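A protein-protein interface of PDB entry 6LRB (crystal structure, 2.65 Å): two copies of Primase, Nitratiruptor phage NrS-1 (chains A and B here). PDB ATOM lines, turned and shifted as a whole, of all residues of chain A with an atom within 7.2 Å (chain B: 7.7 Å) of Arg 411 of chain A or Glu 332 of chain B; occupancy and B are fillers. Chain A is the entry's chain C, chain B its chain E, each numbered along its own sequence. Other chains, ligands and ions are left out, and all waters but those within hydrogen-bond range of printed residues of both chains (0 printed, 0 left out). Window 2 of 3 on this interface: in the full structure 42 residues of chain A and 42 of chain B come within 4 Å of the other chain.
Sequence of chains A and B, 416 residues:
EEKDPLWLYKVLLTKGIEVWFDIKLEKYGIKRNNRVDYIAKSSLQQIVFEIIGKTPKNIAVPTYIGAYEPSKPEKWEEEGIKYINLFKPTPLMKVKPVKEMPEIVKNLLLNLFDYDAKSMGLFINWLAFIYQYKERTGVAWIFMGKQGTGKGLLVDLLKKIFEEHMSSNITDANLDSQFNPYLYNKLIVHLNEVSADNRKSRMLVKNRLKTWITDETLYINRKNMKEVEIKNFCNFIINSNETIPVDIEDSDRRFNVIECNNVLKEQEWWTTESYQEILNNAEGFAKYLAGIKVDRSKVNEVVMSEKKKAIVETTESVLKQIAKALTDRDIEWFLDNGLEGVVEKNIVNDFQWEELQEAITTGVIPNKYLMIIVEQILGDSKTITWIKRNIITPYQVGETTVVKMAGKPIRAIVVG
The side-chain carboxylate (OD1) of Asp 336 of chain B is in hydrogen-bond range of the side-chain hydroxyl (OG1) of Thr 400 of chain A. The guanidinium group (NH2) of Arg 411 of chain A is in salt-bridge range of the side-chain carboxylate (OD2) of Asp 336 of chain B (3.4 Å). The side-chain carboxylate (OE1) of Glu 332 of chain B lies within salt-bridge range of the guanidinium group (NH1) of Arg 411 of chain A (2.8 Å).
N of Asn 367 of chain A is in hydrogen-bond range of O of Arg 411 of chain A. N of Glu 332 of chain B lies within hydrogen-bond range of OD1 of Asp 330 of chain B. N of Thr 401 of chain A sits at hydrogen-bond distance from O of Ala 412 of chain A (2.7 Å). The backbone carbonyl oxygen of Trp 333 of chain B is in hydrogen-bond range of the side-chain amide nitrogen of Asn 337 of chain B (2.9 Å).
O of Leu 335 of chain B touches ND2 of Asn 367 of chain A, 3.9 Å away. Ile 384 of chain A touches Asp 336 of chain B (CG2 to O, 3.4 Å). CG2 of Ile 384 of chain A touches CA of Asn 337 of chain B (3.7 Å). Thr 401 of chain A touches Asp 336 of chain B. Leu 335 of chain B touches Arg 411 of chain A.
Arg 411 of chain A touches three residues of chain B. Glu 332 of chain B touches just one residue of chain A: Arg 411 (2.8 Å). Printed residues of chain A within 4 Å of Asn 337 of chain B: Ile 384 (3.7 Å). Of the printed residues of chain B, Thr 400 of chain A touches Asp 336. Printed residues of chain B within 4 Å of Thr 401 of chain A: Asp 336 (3.9 Å). Lys 368 of chain A touches none of the printed residues of chain B. The nearest residue of chain A that does not touch Glu 332 of chain B is Val 402 of chain A (4.9 Å). The nearest printed residue of chain B that does not touch Asn 367 of chain A is Asp 336 of chain B (4.03 Å).
Of the 17 printed residues of chain A, 5 touch a printed residue of chain B. Hydrophobic or aromatic side chains of chain A that line the printed part of chain B: Ile 384. Along chain B the printed residues that touch a printed residue of chain A span positions 332 to 337. Among the printed residues, 8 pairs touch across the chains.
No position is printed for both chains. Of the 8 pairs that touch across the chains among the printed residues, none has its exchanged pair printed and touching as well.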
ATOM      1  N   ILE A 365      12.653  16.014  15.528  1.00  0.00           N
ATOM      2  CA  ILE A 365      11.449  16.623  16.094  1.00  0.00           C
ATOM      3  C   ILE A 365      10.969  17.751  15.200  1.00  0.00           C
ATOM      4  O   ILE A 365      11.603  18.783  15.120  1.00  0.00           O
ATOM      5  CB  ILE A 365      11.660  17.166  17.529  1.00  0.00           C
ATOM      6  CG1 ILE A 365      12.488  16.199  18.373  1.00  0.00           C
ATOM      7  CG2 ILE A 365      10.312  17.394  18.213  1.00  0.00           C
ATOM      8  CD1 ILE A 365      13.151  16.847  19.564  1.00  0.00           C
ATOM      9  N   PRO A 366       9.837  17.554  14.528  1.00  0.00           N
ATOM     10  CA  PRO A 366       9.172  18.629  13.816  1.00  0.00           C
ATOM     11  C   PRO A 366       8.787  19.793  14.691  1.00  0.00           C
ATOM     12  O   PRO A 366       8.335  19.590  15.828  1.00  0.00           O
ATOM     13  CB  PRO A 366       7.907  17.959  13.300  1.00  0.00           C
ATOM     14  CG  PRO A 366       8.343  16.547  13.079  1.00  0.00           C
ATOM     15  CD  PRO A 366       9.223  16.251  14.244  1.00  0.00           C
ATOM     16  N   ASN A 367       8.956  21.001  14.156  1.00  0.00           N
ATOM     17  CA  ASN A 367       8.590  22.219  14.860  1.00  0.00           C
ATOM     18  C   ASN A 367       7.235  22.055  15.553  1.00  0.00           C
ATOM     19  O   ASN A 367       7.158  22.151  16.781  1.00  0.00           O
ATOM     20  CB  ASN A 367       8.567  23.420  13.911  1.00  0.00           C
ATOM     21  CG  ASN A 367       9.947  24.041  13.694  1.00  0.00           C
ATOM     22  OD1 ASN A 367      10.949  23.654  14.308  1.00  0.00           O
ATOM     23  ND2 ASN A 367       9.995  25.032  12.811  1.00  0.00           N
ATOM     24  N   LYS A 368       6.189  21.733  14.794  1.00  0.00           N
ATOM     25  CA  LYS A 368       4.851  21.670  15.385  1.00  0.00           C
ATOM     26  C   LYS A 368       4.682  20.606  16.484  1.00  0.00           C
ATOM     27  O   LYS A 368       3.713  20.649  17.224  1.00  0.00           O
ATOM     28  CB  LYS A 368       3.753  21.546  14.311  1.00  0.00           C
ATOM     29  CG  LYS A 368       3.567  20.172  13.674  1.00  0.00           C
ATOM     30  CD  LYS A 368       2.180  20.024  13.043  1.00  0.00           C
ATOM     31  CE  LYS A 368       1.823  18.565  12.802  1.00  0.00           C
ATOM     32  NZ  LYS A 368       2.846  17.861  11.974  1.00  0.00           N
ATOM     33  N   TYR A 369       5.597  19.644  16.567  1.00  0.00           N
ATOM     34  CA  TYR A 369       5.622  18.697  17.688  1.00  0.00           C
ATOM     35  C   TYR A 369       6.442  19.239  18.856  1.00  0.00           C
ATOM     36  O   TYR A 369       6.066  19.044  20.020  1.00  0.00           O
ATOM     37  CB  TYR A 369       6.132  17.301  17.252  1.00  0.00           C
ATOM     38  CG  TYR A 369       5.162  16.522  16.358  1.00  0.00           C
ATOM     39  CD1 TYR A 369       3.807  16.371  16.702  1.00  0.00           C
ATOM     40  CD2 TYR A 369       5.598  15.910  15.192  1.00  0.00           C
ATOM     41  CE1 TYR A 369       2.930  15.658  15.898  1.00  0.00           C
ATOM     42  CE2 TYR A 369       4.725  15.198  14.380  1.00  0.00           C
ATOM     43  CZ  TYR A 369       3.391  15.070  14.739  1.00  0.00           C
ATOM     44  OH  TYR A 369       2.517  14.362  13.938  1.00  0.00           O
ATOM     45  N   ILE A 384       8.720  28.584  18.693  1.00  0.00           N
ATOM     46  CA  ILE A 384       9.935  27.926  18.246  1.00  0.00           C
ATOM     47  C   ILE A 384      11.111  28.797  18.623  1.00  0.00           C
ATOM     48  O   ILE A 384      12.099  28.293  19.145  1.00  0.00           O
ATOM     49  CB  ILE A 384       9.955  27.709  16.721  1.00  0.00           C
ATOM     50  CG1 ILE A 384       8.920  26.659  16.314  1.00  0.00           C
ATOM     51  CG2 ILE A 384      11.355  27.320  16.229  1.00  0.00           C
ATOM     52  CD1 ILE A 384       9.195  25.251  16.826  1.00  0.00           C
ATOM     53  N   THR A 400      18.487  23.269  14.011  1.00  0.00           N
ATOM     54  CA  THR A 400      17.215  23.427  13.293  1.00  0.00           C
ATOM     55  C   THR A 400      17.460  23.226  11.809  1.00  0.00           C
ATOM     56  O   THR A 400      18.327  23.883  11.227  1.00  0.00           O
ATOM     57  CB  THR A 400      16.540  24.821  13.501  1.00  0.00           C
ATOM     58  OG1 THR A 400      17.479  25.883  13.259  1.00  0.00           O
ATOM     59  CG2 THR A 400      15.993  25.021  14.865  1.00  0.00           C
ATOM     60  N   THR A 401      16.678  22.346  11.187  1.00  0.00           N
ATOM     61  CA  THR A 401      16.939  21.910   9.818  1.00  0.00           C
ATOM     62  C   THR A 401      15.647  21.565   9.107  1.00  0.00           C
ATOM     63  O   THR A 401      14.566  21.684   9.687  1.00  0.00           O
ATOM     64  CB  THR A 401      17.863  20.612   9.761  1.00  0.00           C
ATOM     65  OG1 THR A 401      17.109  19.398   9.591  1.00  0.00           O
ATOM     66  CG2 THR A 401      18.762  20.360  10.992  1.00  0.00           C
ATOM     67  N   VAL A 402      15.763  21.137   7.852  1.00  0.00           N
ATOM     68  CA  VAL A 402      14.628  20.554   7.111  1.00  0.00           C
ATOM     69  C   VAL A 402      14.797  19.014   7.022  1.00  0.00           C
ATOM     70  O   VAL A 402      15.914  18.500   6.850  1.00  0.00           O
ATOM     71  CB  VAL A 402      14.503  21.160   5.692  1.00  0.00           C
ATOM     72  CG1 VAL A 402      13.177  20.795   5.063  1.00  0.00           C
ATOM     73  CG2 VAL A 402      14.592  22.673   5.772  1.00  0.00           C
ATOM     74  N   VAL A 403      13.682  18.299   7.124  1.00  0.00           N
ATOM     75  CA  VAL A 403      13.626  16.916   6.744  1.00  0.00           C
ATOM     76  C   VAL A 403      12.296  16.670   6.009  1.00  0.00           C
ATOM     77  O   VAL A 403      11.292  17.286   6.356  1.00  0.00           O
ATOM     78  CB  VAL A 403      13.748  15.954   8.005  1.00  0.00           C
ATOM     79  CG1 VAL A 403      15.090  16.144   8.696  1.00  0.00           C
ATOM     80  CG2 VAL A 403      12.594  16.111   8.989  1.00  0.00           C
ATOM     81  N   MET A 405       9.264  14.741   5.646  1.00  0.00           N
ATOM     82  CA  MET A 405       8.414  13.735   6.297  1.00  0.00           C
ATOM     83  C   MET A 405       7.161  13.603   5.466  1.00  0.00           C
ATOM     84  O   MET A 405       6.536  14.616   5.119  1.00  0.00           O
ATOM     85  CB  MET A 405       8.033  14.152   7.711  1.00  0.00           C
ATOM     86  CG  MET A 405       8.924  13.580   8.780  1.00  0.00           C
ATOM     87  SD  MET A 405       8.473  14.454  10.270  1.00  0.00           S
ATOM     88  CE  MET A 405       7.820  13.182  11.346  1.00  0.00           C
ATOM     89  N   LYS A 408       5.966  16.241   2.149  1.00  0.00           N
ATOM     90  CA  LYS A 408       6.187  17.635   2.532  1.00  0.00           C
ATOM     91  C   LYS A 408       7.541  17.833   3.256  1.00  0.00           C
ATOM     92  O   LYS A 408       7.931  16.965   4.049  1.00  0.00           O
ATOM     93  CB  LYS A 408       5.036  18.089   3.430  1.00  0.00           C
ATOM     94  N   PRO A 409       8.287  18.934   2.948  1.00  0.00           N
ATOM     95  CA  PRO A 409       9.529  19.254   3.673  1.00  0.00           C
ATOM     96  C   PRO A 409       9.210  20.009   4.945  1.00  0.00           C
ATOM     97  O   PRO A 409       8.548  21.035   4.890  1.00  0.00           O
ATOM     98  CB  PRO A 409      10.314  20.141   2.696  1.00  0.00           C
ATOM     99  CG  PRO A 409       9.277  20.799   1.873  1.00  0.00           C
ATOM    100  CD  PRO A 409       8.067  19.884   1.840  1.00  0.00           C
ATOM    101  N   ILE A 410       9.680  19.475   6.075  1.00  0.00           N
ATOM    102  CA  ILE A 410       9.272  19.896   7.409  1.00  0.00           C
ATOM    103  C   ILE A 410      10.473  20.522   8.092  1.00  0.00           C
ATOM    104  O   ILE A 410      11.568  19.968   8.050  1.00  0.00           O
ATOM    105  CB  ILE A 410       8.767  18.676   8.230  1.00  0.00           C
ATOM    106  CG1 ILE A 410       7.446  18.122   7.656  1.00  0.00           C
ATOM    107  CG2 ILE A 410       8.608  18.998   9.711  1.00  0.00           C
ATOM    108  CD1 ILE A 410       6.243  19.049   7.733  1.00  0.00           C
ATOM    109  N   ARG A 411      10.247  21.659   8.743  1.00  0.00           N
ATOM    110  CA  ARG A 411      11.228  22.239   9.658  1.00  0.00           C
ATOM    111  C   ARG A 411      11.274  21.397  10.929  1.00  0.00           C
ATOM    112  O   ARG A 411      10.226  21.148  11.562  1.00  0.00           O
ATOM    113  CB  ARG A 411      10.849  23.664  10.042  1.00  0.00           C
ATOM    114  CG  ARG A 411      10.929  24.672   8.909  1.00  0.00           C
ATOM    115  CD  ARG A 411      12.368  25.095   8.675  1.00  0.00           C
ATOM    116  NE  ARG A 411      12.541  25.653   7.332  1.00  0.00           N
ATOM    117  CZ  ARG A 411      13.710  26.042   6.811  1.00  0.00           C
ATOM    118  NH1 ARG A 411      13.730  26.588   5.602  1.00  0.00           N
ATOM    119  NH2 ARG A 411      14.855  25.931   7.507  1.00  0.00           N
ATOM    120  N   ALA A 412      12.467  20.958  11.304  1.00  0.00           N
ATOM    121  CA  ALA A 412      12.601  20.096  12.458  1.00  0.00           C
ATOM    122  C   ALA A 412      13.862  20.414  13.207  1.00  0.00           C
ATOM    123  O   ALA A 412      14.775  21.044  12.667  1.00  0.00           O
ATOM    124  CB  ALA A 412      12.604  18.648  12.024  1.00  0.00           C
ATOM    125  N   ILE A 413      13.904  19.951  14.449  1.00  0.00           N
ATOM    126  CA  ILE A 413      15.117  19.990  15.241  1.00  0.00           C
ATOM    127  C   ILE A 413      15.714  18.573  15.282  1.00  0.00           C
ATOM    128  O   ILE A 413      15.043  17.591  15.636  1.00  0.00           O
ATOM    129  CB  ILE A 413      14.916  20.661  16.628  1.00  0.00           C
ATOM    130  CG1 ILE A 413      16.269  20.939  17.362  1.00  0.00           C
ATOM    131  CG2 ILE A 413      13.928  19.910  17.483  1.00  0.00           C
ATOM    132  CD1 ILE A 413      16.944  19.810  18.116  1.00  0.00           C
ATOM    133  N   ALA B 325      18.070  39.281  10.447  1.00  0.00           N
ATOM    134  CA  ALA B 325      17.368  38.502   9.413  1.00  0.00           C
ATOM    135  C   ALA B 325      16.624  39.392   8.404  1.00  0.00           C
ATOM    136  O   ALA B 325      16.555  39.057   7.231  1.00  0.00           O
ATOM    137  CB  ALA B 325      16.407  37.512  10.045  1.00  0.00           C
ATOM    138  N   ARG B 329      18.071  39.857   4.536  1.00  0.00           N
ATOM    139  CA  ARG B 329      16.994  39.361   3.668  1.00  0.00           C
ATOM    140  C   ARG B 329      16.939  37.837   3.732  1.00  0.00           C
ATOM    141  O   ARG B 329      16.817  37.159   2.710  1.00  0.00           O
ATOM    142  CB  ARG B 329      17.166  39.877   2.227  1.00  0.00           C
ATOM    143  CG  ARG B 329      17.000  41.396   2.103  1.00  0.00           C
ATOM    144  CD  ARG B 329      17.673  41.986   0.862  1.00  0.00           C
ATOM    145  NE  ARG B 329      18.364  43.248   1.172  1.00  0.00           N
ATOM    146  CZ  ARG B 329      17.942  44.488   0.885  1.00  0.00           C
ATOM    147  NH1 ARG B 329      16.801  44.718   0.239  1.00  0.00           N
ATOM    148  NH2 ARG B 329      18.689  45.530   1.255  1.00  0.00           N
ATOM    149  N   ASP B 330      17.004  37.325   4.959  1.00  0.00           N
ATOM    150  CA  ASP B 330      17.232  35.912   5.248  1.00  0.00           C
ATOM    151  C   ASP B 330      15.921  35.239   5.672  1.00  0.00           C
ATOM    152  O   ASP B 330      15.659  35.070   6.878  1.00  0.00           O
ATOM    153  CB  ASP B 330      18.306  35.778   6.368  1.00  0.00           C
ATOM    154  CG  ASP B 330      18.624  34.316   6.737  1.00  0.00           C
ATOM    155  OD1 ASP B 330      17.976  33.385   6.199  1.00  0.00           O
ATOM    156  OD2 ASP B 330      19.545  34.107   7.543  1.00  0.00           O
ATOM    157  N   ILE B 331      15.128  34.824   4.690  1.00  0.00           N
ATOM    158  CA  ILE B 331      13.905  34.063   4.954  1.00  0.00           C
ATOM    159  C   ILE B 331      14.188  32.802   5.803  1.00  0.00           C
ATOM    160  O   ILE B 331      13.439  32.519   6.753  1.00  0.00           O
ATOM    161  CB  ILE B 331      13.152  33.718   3.646  1.00  0.00           C
ATOM    162  CG1 ILE B 331      11.810  33.031   3.916  1.00  0.00           C
ATOM    163  CG2 ILE B 331      13.986  32.844   2.715  1.00  0.00           C
ATOM    164  CD1 ILE B 331      10.759  33.929   4.524  1.00  0.00           C
ATOM    165  N   GLU B 332      15.283  32.097   5.507  1.00  0.00           N
ATOM    166  CA  GLU B 332      15.554  30.788   6.118  1.00  0.00           C
ATOM    167  C   GLU B 332      15.494  30.835   7.637  1.00  0.00           C
ATOM    168  O   GLU B 332      14.895  29.963   8.269  1.00  0.00           O
ATOM    169  CB  GLU B 332      16.912  30.214   5.688  1.00  0.00           C
ATOM    170  CG  GLU B 332      16.903  28.688   5.535  1.00  0.00           C
ATOM    171  CD  GLU B 332      16.188  28.218   4.271  1.00  0.00           C
ATOM    172  OE1 GLU B 332      16.094  26.971   4.097  1.00  0.00           O
ATOM    173  OE2 GLU B 332      15.696  29.066   3.456  1.00  0.00           O
ATOM    174  N   TRP B 333      16.087  31.877   8.206  1.00  0.00           N
ATOM    175  CA  TRP B 333      16.027  32.136   9.644  1.00  0.00           C
ATOM    176  C   TRP B 333      14.584  32.163  10.147  1.00  0.00           C
ATOM    177  O   TRP B 333      14.218  31.390  11.025  1.00  0.00           O
ATOM    178  CB  TRP B 333      16.715  33.450   9.948  1.00  0.00           C
ATOM    179  CG  TRP B 333      16.916  33.703  11.377  1.00  0.00           C
ATOM    180  CD1 TRP B 333      18.003  33.378  12.118  1.00  0.00           C
ATOM    181  CD2 TRP B 333      16.008  34.374  12.259  1.00  0.00           C
ATOM    182  NE1 TRP B 333      17.830  33.802  13.413  1.00  0.00           N
ATOM    183  CE2 TRP B 333      16.612  34.414  13.523  1.00  0.00           C
ATOM    184  CE3 TRP B 333      14.733  34.945  12.098  1.00  0.00           C
ATOM    185  CZ2 TRP B 333      15.990  35.002  14.623  1.00  0.00           C
ATOM    186  CZ3 TRP B 333      14.113  35.526  13.196  1.00  0.00           C
ATOM    187  CH2 TRP B 333      14.738  35.546  14.438  1.00  0.00           C
ATOM    188  N   PHE B 334      13.754  33.010   9.550  1.00  0.00           N
ATOM    189  CA  PHE B 334      12.333  33.116   9.944  1.00  0.00           C
ATOM    190  C   PHE B 334      11.578  31.800   9.873  1.00  0.00           C
ATOM    191  O   PHE B 334      10.784  31.491  10.756  1.00  0.00           O
ATOM    192  CB  PHE B 334      11.599  34.146   9.092  1.00  0.00           C
ATOM    193  CG  PHE B 334      11.959  35.546   9.429  1.00  0.00           C
ATOM    194  CD1 PHE B 334      11.423  36.144  10.542  1.00  0.00           C
ATOM    195  CD2 PHE B 334      12.875  36.253   8.651  1.00  0.00           C
ATOM    196  CE1 PHE B 334      11.774  37.429  10.882  1.00  0.00           C
ATOM    197  CE2 PHE B 334      13.228  37.545   8.988  1.00  0.00           C
ATOM    198  CZ  PHE B 334      12.676  38.132  10.104  1.00  0.00           C
ATOM    199  N   LEU B 335      11.860  31.012   8.840  1.00  0.00           N
ATOM    200  CA  LEU B 335      11.277  29.682   8.727  1.00  0.00           C
ATOM    201  C   LEU B 335      11.840  28.714   9.791  1.00  0.00           C
ATOM    202  O   LEU B 335      11.089  27.909  10.345  1.00  0.00           O
ATOM    203  CB  LEU B 335      11.490  29.126   7.323  1.00  0.00           C
ATOM    204  CG  LEU B 335      10.674  29.828   6.236  1.00  0.00           C
ATOM    205  CD1 LEU B 335      11.311  29.598   4.879  1.00  0.00           C
ATOM    206  CD2 LEU B 335       9.223  29.353   6.226  1.00  0.00           C
ATOM    207  N   ASP B 336      13.153  28.809  10.055  1.00  0.00           N
ATOM    208  CA  ASP B 336      13.830  28.080  11.155  1.00  0.00           C
ATOM    209  C   ASP B 336      13.206  28.379  12.524  1.00  0.00           C
ATOM    210  O   ASP B 336      13.134  27.493  13.377  1.00  0.00           O
ATOM    211  CB  ASP B 336      15.338  28.414  11.211  1.00  0.00           C
ATOM    212  CG  ASP B 336      16.186  27.412  10.472  1.00  0.00           C
ATOM    213  OD1 ASP B 336      16.163  26.225  10.862  1.00  0.00           O
ATOM    214  OD2 ASP B 336      16.907  27.804   9.540  1.00  0.00           O
ATOM    215  N   ASN B 337      12.772  29.631  12.701  1.00  0.00           N
ATOM    216  CA  ASN B 337      12.034  30.083  13.875  1.00  0.00           C
ATOM    217  C   ASN B 337      10.502  30.097  13.631  1.00  0.00           C
ATOM    218  O   ASN B 337       9.789  30.954  14.152  1.00  0.00           O
ATOM    219  CB  ASN B 337      12.519  31.478  14.315  1.00  0.00           C
ATOM    220  CG  ASN B 337      13.971  31.492  14.778  1.00  0.00           C
ATOM    221  OD1 ASN B 337      14.247  31.540  15.981  1.00  0.00           O
ATOM    222  ND2 ASN B 337      14.900  31.482  13.835  1.00  0.00           N
ATOM    223  N   GLY B 338      10.000  29.142  12.857  1.00  0.00           N
ATOM    224  CA  GLY B 338       8.572  28.837  12.837  1.00  0.00           C
ATOM    225  C   GLY B 338       7.613  29.875  12.278  1.00  0.00           C
ATOM    226  O   GLY B 338       6.448  29.925  12.698  1.00  0.00           O
ATOM    227  N   LEU B 339       8.070  30.668  11.307  1.00  0.00           N
ATOM    228  CA  LEU B 339       7.181  31.589  10.579  1.00  0.00           C
ATOM    229  C   LEU B 339       6.105  30.855   9.760  1.00  0.00           C
ATOM    230  O   LEU B 339       4.980  31.350   9.594  1.00  0.00           O
ATOM    231  CB  LEU B 339       7.980  32.468   9.635  1.00  0.00           C
ATOM    232  CG  LEU B 339       7.179  33.511   8.854  1.00  0.00           C
ATOM    233  CD1 LEU B 339       6.512  34.486   9.800  1.00  0.00           C
ATOM    234  CD2 LEU B 339       8.075  34.260   7.873  1.00  0.00           C
ATOM    235  N   GLU B 340       6.454  29.677   9.260  1.00  0.00           N
ATOM    236  CA  GLU B 340       5.545  28.839   8.460  1.00  0.00           C
ATOM    237  C   GLU B 340       4.207  28.575   9.214  1.00  0.00           C
ATOM    238  O   GLU B 340       3.182  28.260   8.590  1.00  0.00           O
ATOM    239  CB  GLU B 340       6.272  27.536   8.049  1.00  0.00           C
ATOM    240  CG  GLU B 340       5.966  27.009   6.651  1.00  0.00           C
ATOM    241  CD  GLU B 340       4.724  26.143   6.569  1.00  0.00           C
ATOM    242  OE1 GLU B 340       4.249  25.632   7.613  1.00  0.00           O
ATOM    243  OE2 GLU B 340       4.217  25.970   5.437  1.00  0.00           O
ATOM    244  N   ILE B 360      10.263  39.648   2.452  1.00  0.00           N
ATOM    245  CA  ILE B 360      11.433  39.518   3.326  1.00  0.00           C
ATOM    246  C   ILE B 360      12.695  39.487   2.486  1.00  0.00           C
ATOM    247  O   ILE B 360      13.661  40.207   2.777  1.00  0.00           O
ATOM    248  CB  ILE B 360      11.325  38.268   4.240  1.00  0.00           C
ATOM    249  CG1 ILE B 360      10.282  38.531   5.338  1.00  0.00           C
ATOM    250  CG2 ILE B 360      12.655  37.930   4.911  1.00  0.00           C
ATOM    251  CD1 ILE B 360       9.750  37.292   6.025  1.00  0.00           C
ATOM    252  N   THR B 361      12.668  38.636   1.467  1.00  0.00           N
ATOM    253  CA  THR B 361      13.766  38.463   0.513  1.00  0.00           C
ATOM    254  C   THR B 361      14.077  39.737  -0.262  1.00  0.00           C
ATOM    255  O   THR B 361      15.216  40.202  -0.274  1.00  0.00           O
ATOM    256  CB  THR B 361      13.422  37.352  -0.495  1.00  0.00           C
ATOM    257  OG1 THR B 361      12.844  36.245   0.208  1.00  0.00           O
ATOM    258  CG2 THR B 361      14.675  36.896  -1.254  1.00  0.00           C
